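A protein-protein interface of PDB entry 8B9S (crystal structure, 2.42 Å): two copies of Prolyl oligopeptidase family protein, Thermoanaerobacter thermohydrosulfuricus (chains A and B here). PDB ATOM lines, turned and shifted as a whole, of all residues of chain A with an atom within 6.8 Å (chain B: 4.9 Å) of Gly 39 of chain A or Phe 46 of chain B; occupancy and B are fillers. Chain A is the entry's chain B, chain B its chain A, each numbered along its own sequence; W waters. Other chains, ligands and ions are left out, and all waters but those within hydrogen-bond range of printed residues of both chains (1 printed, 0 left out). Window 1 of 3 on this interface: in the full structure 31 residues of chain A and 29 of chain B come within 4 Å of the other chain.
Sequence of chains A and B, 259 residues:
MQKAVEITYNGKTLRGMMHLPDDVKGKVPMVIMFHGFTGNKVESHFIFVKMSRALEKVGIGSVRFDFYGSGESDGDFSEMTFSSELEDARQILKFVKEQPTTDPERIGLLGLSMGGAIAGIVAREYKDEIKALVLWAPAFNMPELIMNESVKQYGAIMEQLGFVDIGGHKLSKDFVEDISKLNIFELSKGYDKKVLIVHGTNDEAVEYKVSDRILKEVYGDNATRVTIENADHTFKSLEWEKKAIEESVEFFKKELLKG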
ATOM      1  N   HIS A  35      24.328   4.336 -38.665  1.00  0.00           N
ATOM      2  CA  HIS A  35      25.454   3.855 -37.883  1.00  0.00           C
ATOM      3  C   HIS A  35      25.273   2.378 -37.527  1.00  0.00           C
ATOM      4  O   HIS A  35      24.211   1.784 -37.729  1.00  0.00           O
ATOM      5  CB  HIS A  35      25.643   4.699 -36.619  1.00  0.00           C
ATOM      6  CG  HIS A  35      24.524   4.582 -35.632  1.00  0.00           C
ATOM      7  ND1 HIS A  35      24.410   3.519 -34.757  1.00  0.00           N
ATOM      8  CD2 HIS A  35      23.489   5.414 -35.351  1.00  0.00           C
ATOM      9  CE1 HIS A  35      23.343   3.692 -33.993  1.00  0.00           C
ATOM     10  NE2 HIS A  35      22.774   4.840 -34.323  1.00  0.00           N
ATOM     11  N   GLY A  36      26.348   1.782 -37.004  1.00  0.00           N
ATOM     12  CA  GLY A  36      26.393   0.368 -36.722  1.00  0.00           C
ATOM     13  C   GLY A  36      26.148  -0.004 -35.263  1.00  0.00           C
ATOM     14  O   GLY A  36      25.812   0.821 -34.407  1.00  0.00           O
ATOM     15  N   PHE A  37      26.347  -1.296 -34.996  1.00  0.00           N
ATOM     16  CA  PHE A  37      25.989  -1.939 -33.736  1.00  0.00           C
ATOM     17  C   PHE A  37      26.881  -1.440 -32.602  1.00  0.00           C
ATOM     18  O   PHE A  37      28.102  -1.640 -32.630  1.00  0.00           O
ATOM     19  CB  PHE A  37      26.097  -3.456 -33.919  1.00  0.00           C
ATOM     20  CG  PHE A  37      25.560  -4.257 -32.763  1.00  0.00           C
ATOM     21  CD1 PHE A  37      24.212  -4.258 -32.473  1.00  0.00           C
ATOM     22  CD2 PHE A  37      26.398  -5.061 -32.009  1.00  0.00           C
ATOM     23  CE1 PHE A  37      23.711  -5.016 -31.424  1.00  0.00           C
ATOM     24  CE2 PHE A  37      25.901  -5.820 -30.961  1.00  0.00           C
ATOM     25  CZ  PHE A  37      24.550  -5.799 -30.675  1.00  0.00           C
ATOM     26  N   THR A  38      26.260  -0.790 -31.613  1.00  0.00           N
ATOM     27  CA  THR A  38      26.854  -0.061 -30.485  1.00  0.00           C
ATOM     28  C   THR A  38      27.503   1.247 -30.913  1.00  0.00           C
ATOM     29  O   THR A  38      28.106   1.927 -30.075  1.00  0.00           O
ATOM     30  CB  THR A  38      27.894  -0.863 -29.679  1.00  0.00           C
ATOM     31  OG1 THR A  38      29.037  -1.147 -30.494  1.00  0.00           O
ATOM     32  CG2 THR A  38      27.303  -2.162 -29.136  1.00  0.00           C
ATOM     33  N   GLY A  39      27.379   1.632 -32.179  1.00  0.00           N
ATOM     34  CA  GLY A  39      27.859   2.920 -32.632  1.00  0.00           C
ATOM     35  C   GLY A  39      26.851   4.023 -32.378  1.00  0.00           C
ATOM     36  O   GLY A  39      25.880   3.874 -31.631  1.00  0.00           O
ATOM     37  N   ASN A  40      27.118   5.173 -32.996  1.00  0.00           N
ATOM     38  CA  ASN A  40      26.226   6.318 -32.882  1.00  0.00           C
ATOM     39  C   ASN A  40      26.482   7.229 -34.078  1.00  0.00           C
ATOM     40  O   ASN A  40      27.453   7.046 -34.813  1.00  0.00           O
ATOM     41  CB  ASN A  40      26.425   6.989 -31.508  1.00  0.00           C
ATOM     42  CG  ASN A  40      27.697   7.836 -31.415  1.00  0.00           C
ATOM     43  OD1 ASN A  40      28.037   8.612 -32.314  1.00  0.00           O
ATOM     44  ND2 ASN A  40      28.472   7.582 -30.372  1.00  0.00           N
ATOM     45  N   LYS A  41      25.629   8.256 -34.223  1.00  0.00           N
ATOM     46  CA  LYS A  41      25.584   9.101 -35.420  1.00  0.00           C
ATOM     47  C   LYS A  41      26.915   9.759 -35.767  1.00  0.00           C
ATOM     48  O   LYS A  41      27.100  10.177 -36.917  1.00  0.00           O
ATOM     49  CB  LYS A  41      24.507  10.171 -35.265  1.00  0.00           C
ATOM     50  CG  LYS A  41      24.668  11.093 -34.086  1.00  0.00           C
ATOM     51  CD  LYS A  41      23.549  12.136 -34.079  1.00  0.00           C
ATOM     52  CE  LYS A  41      23.491  12.935 -32.777  1.00  0.00           C
ATOM     53  NZ  LYS A  41      24.685  13.752 -32.556  1.00  0.00           N
ATOM     54  N   VAL A  42      27.805   9.937 -34.785  1.00  0.00           N
ATOM     55  CA  VAL A  42      29.151  10.438 -35.053  1.00  0.00           C
ATOM     56  C   VAL A  42      30.039   9.358 -35.676  1.00  0.00           C
ATOM     57  O   VAL A  42      30.922   9.663 -36.493  1.00  0.00           O
ATOM     58  CB  VAL A  42      29.741  11.021 -33.756  1.00  0.00           C
ATOM     59  CG1 VAL A  42      31.218  11.212 -33.879  1.00  0.00           C
ATOM     60  CG2 VAL A  42      29.080  12.376 -33.457  1.00  0.00           C
ATOM     61  N   GLU A  43      29.864   8.101 -35.233  1.00  0.00           N
ATOM     62  CA  GLU A  43      30.651   6.921 -35.618  1.00  0.00           C
ATOM     63  C   GLU A  43      32.139   7.017 -35.310  1.00  0.00           C
ATOM     64  O   GLU A  43      32.640   8.040 -34.827  1.00  0.00           O
ATOM     65  CB  GLU A  43      30.488   6.520 -37.081  1.00  0.00           C
ATOM     66  CG  GLU A  43      29.386   5.472 -37.360  1.00  0.00           C
ATOM     67  CD  GLU A  43      29.673   4.109 -36.684  1.00  0.00           C
ATOM     68  OE1 GLU A  43      30.825   3.842 -36.289  1.00  0.00           O
ATOM     69  OE2 GLU A  43      28.755   3.263 -36.603  1.00  0.00           O
ATOM     70  N   SER A  44      32.834   5.927 -35.628  1.00  0.00           N
ATOM     71  CA  SER A  44      34.223   5.722 -35.252  1.00  0.00           C
ATOM     72  C   SER A  44      35.120   6.824 -35.810  1.00  0.00           C
ATOM     73  O   SER A  44      35.018   7.187 -36.985  1.00  0.00           O
ATOM     74  CB  SER A  44      34.667   4.344 -35.756  1.00  0.00           C
ATOM     75  OG  SER A  44      35.964   4.009 -35.321  1.00  0.00           O
ATOM     76  N   ASP A  66      20.799   9.079 -34.235  1.00  0.00           N
ATOM     77  CA  ASP A  66      21.083   7.910 -33.414  1.00  0.00           C
ATOM     78  C   ASP A  66      19.826   7.062 -33.355  1.00  0.00           C
ATOM     79  O   ASP A  66      18.725   7.587 -33.157  1.00  0.00           O
ATOM     80  CB  ASP A  66      21.518   8.308 -31.988  1.00  0.00           C
ATOM     81  CG  ASP A  66      22.871   8.986 -31.926  1.00  0.00           C
ATOM     82  OD1 ASP A  66      23.843   8.442 -32.470  1.00  0.00           O
ATOM     83  OD2 ASP A  66      22.944  10.068 -31.294  1.00  0.00           O
ATOM     84  N   PHE A  67      19.964   5.740 -33.566  1.00  0.00           N
ATOM     85  CA  PHE A  67      18.805   4.865 -33.454  1.00  0.00           C
ATOM     86  C   PHE A  67      18.281   4.865 -32.019  1.00  0.00           C
ATOM     87  O   PHE A  67      18.990   5.200 -31.069  1.00  0.00           O
ATOM     88  CB  PHE A  67      19.141   3.442 -33.917  1.00  0.00           C
ATOM     89  CG  PHE A  67      19.336   3.320 -35.412  1.00  0.00           C
ATOM     90  CD1 PHE A  67      18.252   3.447 -36.276  1.00  0.00           C
ATOM     91  CD2 PHE A  67      20.584   3.040 -35.950  1.00  0.00           C
ATOM     92  CE1 PHE A  67      18.424   3.342 -37.656  1.00  0.00           C
ATOM     93  CE2 PHE A  67      20.761   2.913 -37.336  1.00  0.00           C
ATOM     94  CZ  PHE A  67      19.690   3.067 -38.183  1.00  0.00           C
ATOM     95  N   GLY A  69      17.581   3.879 -28.477  1.00  0.00           N
ATOM     96  CA  GLY A  69      18.414   3.056 -27.618  1.00  0.00           C
ATOM     97  C   GLY A  69      19.908   3.311 -27.697  1.00  0.00           C
ATOM     98  O   GLY A  69      20.665   2.636 -26.990  1.00  0.00           O
ATOM     99  N   SER A  70      20.359   4.238 -28.550  1.00  0.00           N
ATOM    100  CA  SER A  70      21.775   4.554 -28.691  1.00  0.00           C
ATOM    101  C   SER A  70      22.013   6.061 -28.629  1.00  0.00           C
ATOM    102  O   SER A  70      21.140   6.864 -28.987  1.00  0.00           O
ATOM    103  CB  SER A  70      22.346   4.014 -30.017  1.00  0.00           C
ATOM    104  OG  SER A  70      22.318   2.590 -30.058  1.00  0.00           O
ATOM    105  N   GLY A  71      23.224   6.433 -28.203  1.00  0.00           N
ATOM    106  CA  GLY A  71      23.699   7.809 -28.213  1.00  0.00           C
ATOM    107  C   GLY A  71      22.806   8.866 -27.581  1.00  0.00           C
ATOM    108  O   GLY A  71      22.411   8.759 -26.419  1.00  0.00           O
ATOM    109  N   GLU A  72      22.470   9.903 -28.355  1.00  0.00           N
ATOM    110  CA  GLU A  72      21.650  10.992 -27.842  1.00  0.00           C
ATOM    111  C   GLU A  72      20.149  10.702 -27.881  1.00  0.00           C
ATOM    112  O   GLU A  72      19.380  11.435 -27.240  1.00  0.00           O
ATOM    113  CB  GLU A  72      21.931  12.275 -28.619  1.00  0.00           C
ATOM    114  CG  GLU A  72      23.334  12.860 -28.478  1.00  0.00           C
ATOM    115  CD  GLU A  72      23.652  13.320 -27.057  1.00  0.00           C
ATOM    116  OE1 GLU A  72      22.711  13.428 -26.242  1.00  0.00           O
ATOM    117  OE2 GLU A  72      24.827  13.650 -26.784  1.00  0.00           O
ATOM    118  N   PHE A  77      19.373   0.546 -24.475  1.00  0.00           N
ATOM    119  CA  PHE A  77      19.838  -0.383 -25.500  1.00  0.00           C
ATOM    120  C   PHE A  77      19.074  -1.702 -25.433  1.00  0.00           C
ATOM    121  O   PHE A  77      18.878  -2.360 -26.461  1.00  0.00           O
ATOM    122  CB  PHE A  77      21.339  -0.632 -25.326  1.00  0.00           C
ATOM    123  CG  PHE A  77      22.009  -1.252 -26.534  1.00  0.00           C
ATOM    124  CD1 PHE A  77      22.416  -0.454 -27.591  1.00  0.00           C
ATOM    125  CD2 PHE A  77      22.241  -2.622 -26.604  1.00  0.00           C
ATOM    126  CE1 PHE A  77      23.043  -0.996 -28.693  1.00  0.00           C
ATOM    127  CE2 PHE A  77      22.866  -3.184 -27.714  1.00  0.00           C
ATOM    128  CZ  PHE A  77      23.268  -2.368 -28.761  1.00  0.00           C
ATOM    129  N   GLY A 168      29.210  -2.642 -21.509  1.00  0.00           N
ATOM    130  CA  GLY A 168      28.482  -1.463 -21.098  1.00  0.00           C
ATOM    131  C   GLY A 168      27.163  -1.295 -21.808  1.00  0.00           C
ATOM    132  O   GLY A 168      26.554  -0.219 -21.725  1.00  0.00           O
ATOM    133  N   HIS A 169      26.681  -2.343 -22.465  1.00  0.00           N
ATOM    134  CA  HIS A 169      25.392  -2.338 -23.136  1.00  0.00           C
ATOM    135  C   HIS A 169      24.644  -3.605 -22.748  1.00  0.00           C
ATOM    136  O   HIS A 169      25.249  -4.674 -22.625  1.00  0.00           O
ATOM    137  CB  HIS A 169      25.554  -2.281 -24.660  1.00  0.00           C
ATOM    138  CG  HIS A 169      26.359  -1.118 -25.156  1.00  0.00           C
ATOM    139  ND1 HIS A 169      25.883   0.177 -25.155  1.00  0.00           N
ATOM    140  CD2 HIS A 169      27.598  -1.065 -25.710  1.00  0.00           C
ATOM    141  CE1 HIS A 169      26.801   0.977 -25.672  1.00  0.00           C
ATOM    142  NE2 HIS A 169      27.847   0.249 -26.018  1.00  0.00           N
ATOM    143  N   VAL B  42      29.038  12.024 -25.815  1.00  0.00           N
ATOM    144  CA  VAL B  42      28.307  10.824 -25.426  1.00  0.00           C
ATOM    145  C   VAL B  42      29.176   9.915 -24.564  1.00  0.00           C
ATOM    146  O   VAL B  42      28.681   9.254 -23.642  1.00  0.00           O
ATOM    147  CB  VAL B  42      27.769  10.111 -26.682  1.00  0.00           C
ATOM    148  CG1 VAL B  42      27.277   8.740 -26.354  1.00  0.00           C
ATOM    149  CG2 VAL B  42      26.622  10.911 -27.290  1.00  0.00           C
ATOM    150  N   GLU B  43      30.473   9.850 -24.885  1.00  0.00           N
ATOM    151  CA  GLU B  43      31.483   8.976 -24.276  1.00  0.00           C
ATOM    152  C   GLU B  43      31.219   7.482 -24.413  1.00  0.00           C
ATOM    153  O   GLU B  43      30.187   7.044 -24.936  1.00  0.00           O
ATOM    154  CB  GLU B  43      31.744   9.284 -22.807  1.00  0.00           C
ATOM    155  CG  GLU B  43      32.884  10.291 -22.570  1.00  0.00           C
ATOM    156  CD  GLU B  43      34.245   9.759 -23.087  1.00  0.00           C
ATOM    157  OE1 GLU B  43      34.371   8.517 -23.293  1.00  0.00           O
ATOM    158  OE2 GLU B  43      35.202  10.569 -23.242  1.00  0.00           O
ATOM    159  N   SER B  44      32.179   6.716 -23.903  1.00  0.00           N
ATOM    160  CA  SER B  44      32.244   5.272 -24.088  1.00  0.00           C
ATOM    161  C   SER B  44      31.004   4.571 -23.538  1.00  0.00           C
ATOM    162  O   SER B  44      30.581   4.804 -22.392  1.00  0.00           O
ATOM    163  CB  SER B  44      33.516   4.755 -23.410  1.00  0.00           C
ATOM    164  OG  SER B  44      33.648   3.358 -23.559  1.00  0.00           O
ATOM    165  N   HIS B  45      30.442   3.677 -24.359  1.00  0.00           N
ATOM    166  CA  HIS B  45      29.183   2.987 -24.083  1.00  0.00           C
ATOM    167  C   HIS B  45      28.170   3.957 -23.475  1.00  0.00           C
ATOM    168  O   HIS B  45      27.446   3.624 -22.533  1.00  0.00           O
ATOM    169  CB  HIS B  45      29.416   1.735 -23.211  1.00  0.00           C
ATOM    170  CG  HIS B  45      30.227   1.987 -21.974  1.00  0.00           C
ATOM    171  ND1 HIS B  45      29.663   2.299 -20.757  1.00  0.00           N
ATOM    172  CD2 HIS B  45      31.568   2.015 -21.786  1.00  0.00           C
ATOM    173  CE1 HIS B  45      30.622   2.487 -19.867  1.00  0.00           C
ATOM    174  NE2 HIS B  45      31.787   2.320 -20.467  1.00  0.00           N
ATOM    175  N   PHE B  46      28.133   5.173 -24.019  1.00  0.00           N
ATOM    176  CA  PHE B  46      27.089   6.158 -23.752  1.00  0.00           C
ATOM    177  C   PHE B  46      27.081   6.592 -22.293  1.00  0.00           C
ATOM    178  O   PHE B  46      26.086   7.142 -21.822  1.00  0.00           O
ATOM    179  CB  PHE B  46      25.711   5.604 -24.129  1.00  0.00           C
ATOM    180  CG  PHE B  46      25.632   5.048 -25.535  1.00  0.00           C
ATOM    181  CD1 PHE B  46      26.449   5.515 -26.542  1.00  0.00           C
ATOM    182  CD2 PHE B  46      24.790   3.983 -25.815  1.00  0.00           C
ATOM    183  CE1 PHE B  46      26.380   4.972 -27.814  1.00  0.00           C
ATOM    184  CE2 PHE B  46      24.729   3.434 -27.079  1.00  0.00           C
ATOM    185  CZ  PHE B  46      25.518   3.931 -28.076  1.00  0.00           C
ATOM    186  N   ILE B  47      28.182   6.367 -21.569  1.00  0.00           N
ATOM    187  CA  ILE B  47      28.149   6.537 -20.118  1.00  0.00           C
ATOM    188  C   ILE B  47      27.784   7.970 -19.735  1.00  0.00           C
ATOM    189  O   ILE B  47      27.149   8.197 -18.696  1.00  0.00           O
ATOM    190  CB  ILE B  47      29.476   6.081 -19.475  1.00  0.00           C
ATOM    191  CG1 ILE B  47      29.314   6.036 -17.954  1.00  0.00           C
ATOM    192  CG2 ILE B  47      30.644   6.959 -19.921  1.00  0.00           C
ATOM    193  CD1 ILE B  47      30.459   5.334 -17.207  1.00  0.00           C
ATOM    194  N   PHE B  48      28.162   8.959 -20.557  1.00  0.00           N
ATOM    195  CA  PHE B  48      27.767  10.329 -20.254  1.00  0.00           C
ATOM    196  C   PHE B  48      26.263  10.539 -20.387  1.00  0.00           C
ATOM    197  O   PHE B  48      25.648  11.175 -19.520  1.00  0.00           O
ATOM    198  CB  PHE B  48      28.503  11.332 -21.136  1.00  0.00           C
ATOM    199  CG  PHE B  48      29.803  11.790 -20.575  1.00  0.00           C
ATOM    200  CD1 PHE B  48      30.286  11.261 -19.384  1.00  0.00           C
ATOM    201  CD2 PHE B  48      30.472  12.858 -21.161  1.00  0.00           C
ATOM    202  CE1 PHE B  48      31.477  11.709 -18.848  1.00  0.00           C
ATOM    203  CE2 PHE B  48      31.663  13.327 -20.633  1.00  0.00           C
ATOM    204  CZ  PHE B  48      32.173  12.751 -19.465  1.00  0.00           C
ATOM    205  N   VAL B  49      25.653  10.032 -21.466  1.00  0.00           N
ATOM    206  CA  VAL B  49      24.208  10.177 -21.627  1.00  0.00           C
ATOM    207  C   VAL B  49      23.516   9.583 -20.416  1.00  0.00           C
ATOM    208  O   VAL B  49      22.716  10.235 -19.742  1.00  0.00           O
ATOM    209  CB  VAL B  49      23.726   9.508 -22.931  1.00  0.00           C
ATOM    210  CG1 VAL B  49      22.248   9.747 -23.119  1.00  0.00           C
ATOM    211  CG2 VAL B  49      24.508  10.000 -24.151  1.00  0.00           C
ATOM    212  N   LYS B  50      23.908   8.361 -20.066  1.00  0.00           N
ATOM    213  CA  LYS B  50      23.376   7.697 -18.885  1.00  0.00           C
ATOM    214  C   LYS B  50      23.507   8.586 -17.659  1.00  0.00           C
ATOM    215  O   LYS B  50      22.535   8.778 -16.914  1.00  0.00           O
ATOM    216  CB  LYS B  50      24.113   6.372 -18.691  1.00  0.00           C
ATOM    217  CG  LYS B  50      23.801   5.360 -19.795  1.00  0.00           C
ATOM    218  CD  LYS B  50      24.731   4.146 -19.756  1.00  0.00           C
ATOM    219  CE  LYS B  50      24.415   3.196 -20.897  1.00  0.00           C
ATOM    220  NZ  LYS B  50      25.422   2.133 -21.087  1.00  0.00           N
HETATM  221  O   HOH W   1      23.630   1.382 -23.466  1.00  0.00           O
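Among the printed residues, pairs that only touch across the chains: Glu 72 of chain A with Val 42 of chain B (3.3 Å), Gly 71 of chain A with Val 49 of chain B (3.3 Å), Gly 71 of chain A with Phe 46 of chain B (3.4 Å), His 169 of chain A with His 45 of chain B (3.5 Å), His 169 of chain A with Phe 46 of chain B (3.5 Å), Ser 70 of chain A with Phe 46 of chain B (3.5 Å), Gly 39 of chain A with Phe 46 of chain B (3.6 Å), Gly 168 of chain A with His 45 of chain B (3.8 Å) and Thr 38 of chain A with Phe 46 of chain B (3.8 Å).
Positions printed for both chains: 42, 43 and 44.
Of the 10 pairs that touch across the chains among the printed residues, none has its exchanged pair printed and touching as well.
Phe 67 of chain A touches none of the printed residues of chain B.
Printed residues of chain B within 4 Å of Glu 72 of chain A: Val 42.
Printed residues of chain A within 4 Å of Val 42 of chain B: Glu 72 (3.3 Å).
Glu 43 of chain B touches none of the printed residues of chain A.
Phe 46 of chain B touches just these residues of chain A: Thr 38 (3.8 Å), Gly 39 (3.6 Å), Ser 70 (3.5 Å), Gly 71 (3.4 Å) and His 169 (3.5 Å).
Of the printed residues of chain A, Val 49 of chain B touches Gly 71 (3.3 Å).
Printed residues of chain A within 4 Å of Lys 50 of chain B: Gly 168 (2.7 Å).
The nearest printed residue of chain B that does not touch Gly 39 of chain A is Val 42 of chain B (7.3 Å).
The nearest printed residue of chain A that does not touch Val 49 of chain B is Glu 72 of chain A (4.4 Å).
Water W1 bridges a ring nitrogen (ND1) of His 169 of chain A (3.1 Å) and the side-chain amino group (NZ) of Lys 50 of chain B (3.1 Å).
The backbone carbonyl oxygen (O) of Gly 168 of chain A lies within hydrogen-bond range of the side-chain amino group (NZ) of Lys 50 of chain B (2.7 Å).
The backbone carbonyl oxygen (O) of Val 42 of chain B is in hydrogen-bond range of the backbone NH (N) of Phe 48 of chain B, 3.1 Å away.
The backbone carbonyl oxygen of His 45 of chain B is in hydrogen-bond range of the side-chain amino group of Lys 50 of chain B (2.9 Å).
A ring nitrogen (ND1) of His 35 of chain A sits close to the backbone carbonyl oxygen of Gly 39 of chain A.
The backbone NH of Glu 72 of chain A lies within hydrogen-bond range of the side-chain carboxylate of Asp 66 of chain A, at 3.0 Å.
Of the 9 printed residues of chain B, 5 touch a printed residue of chain A.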
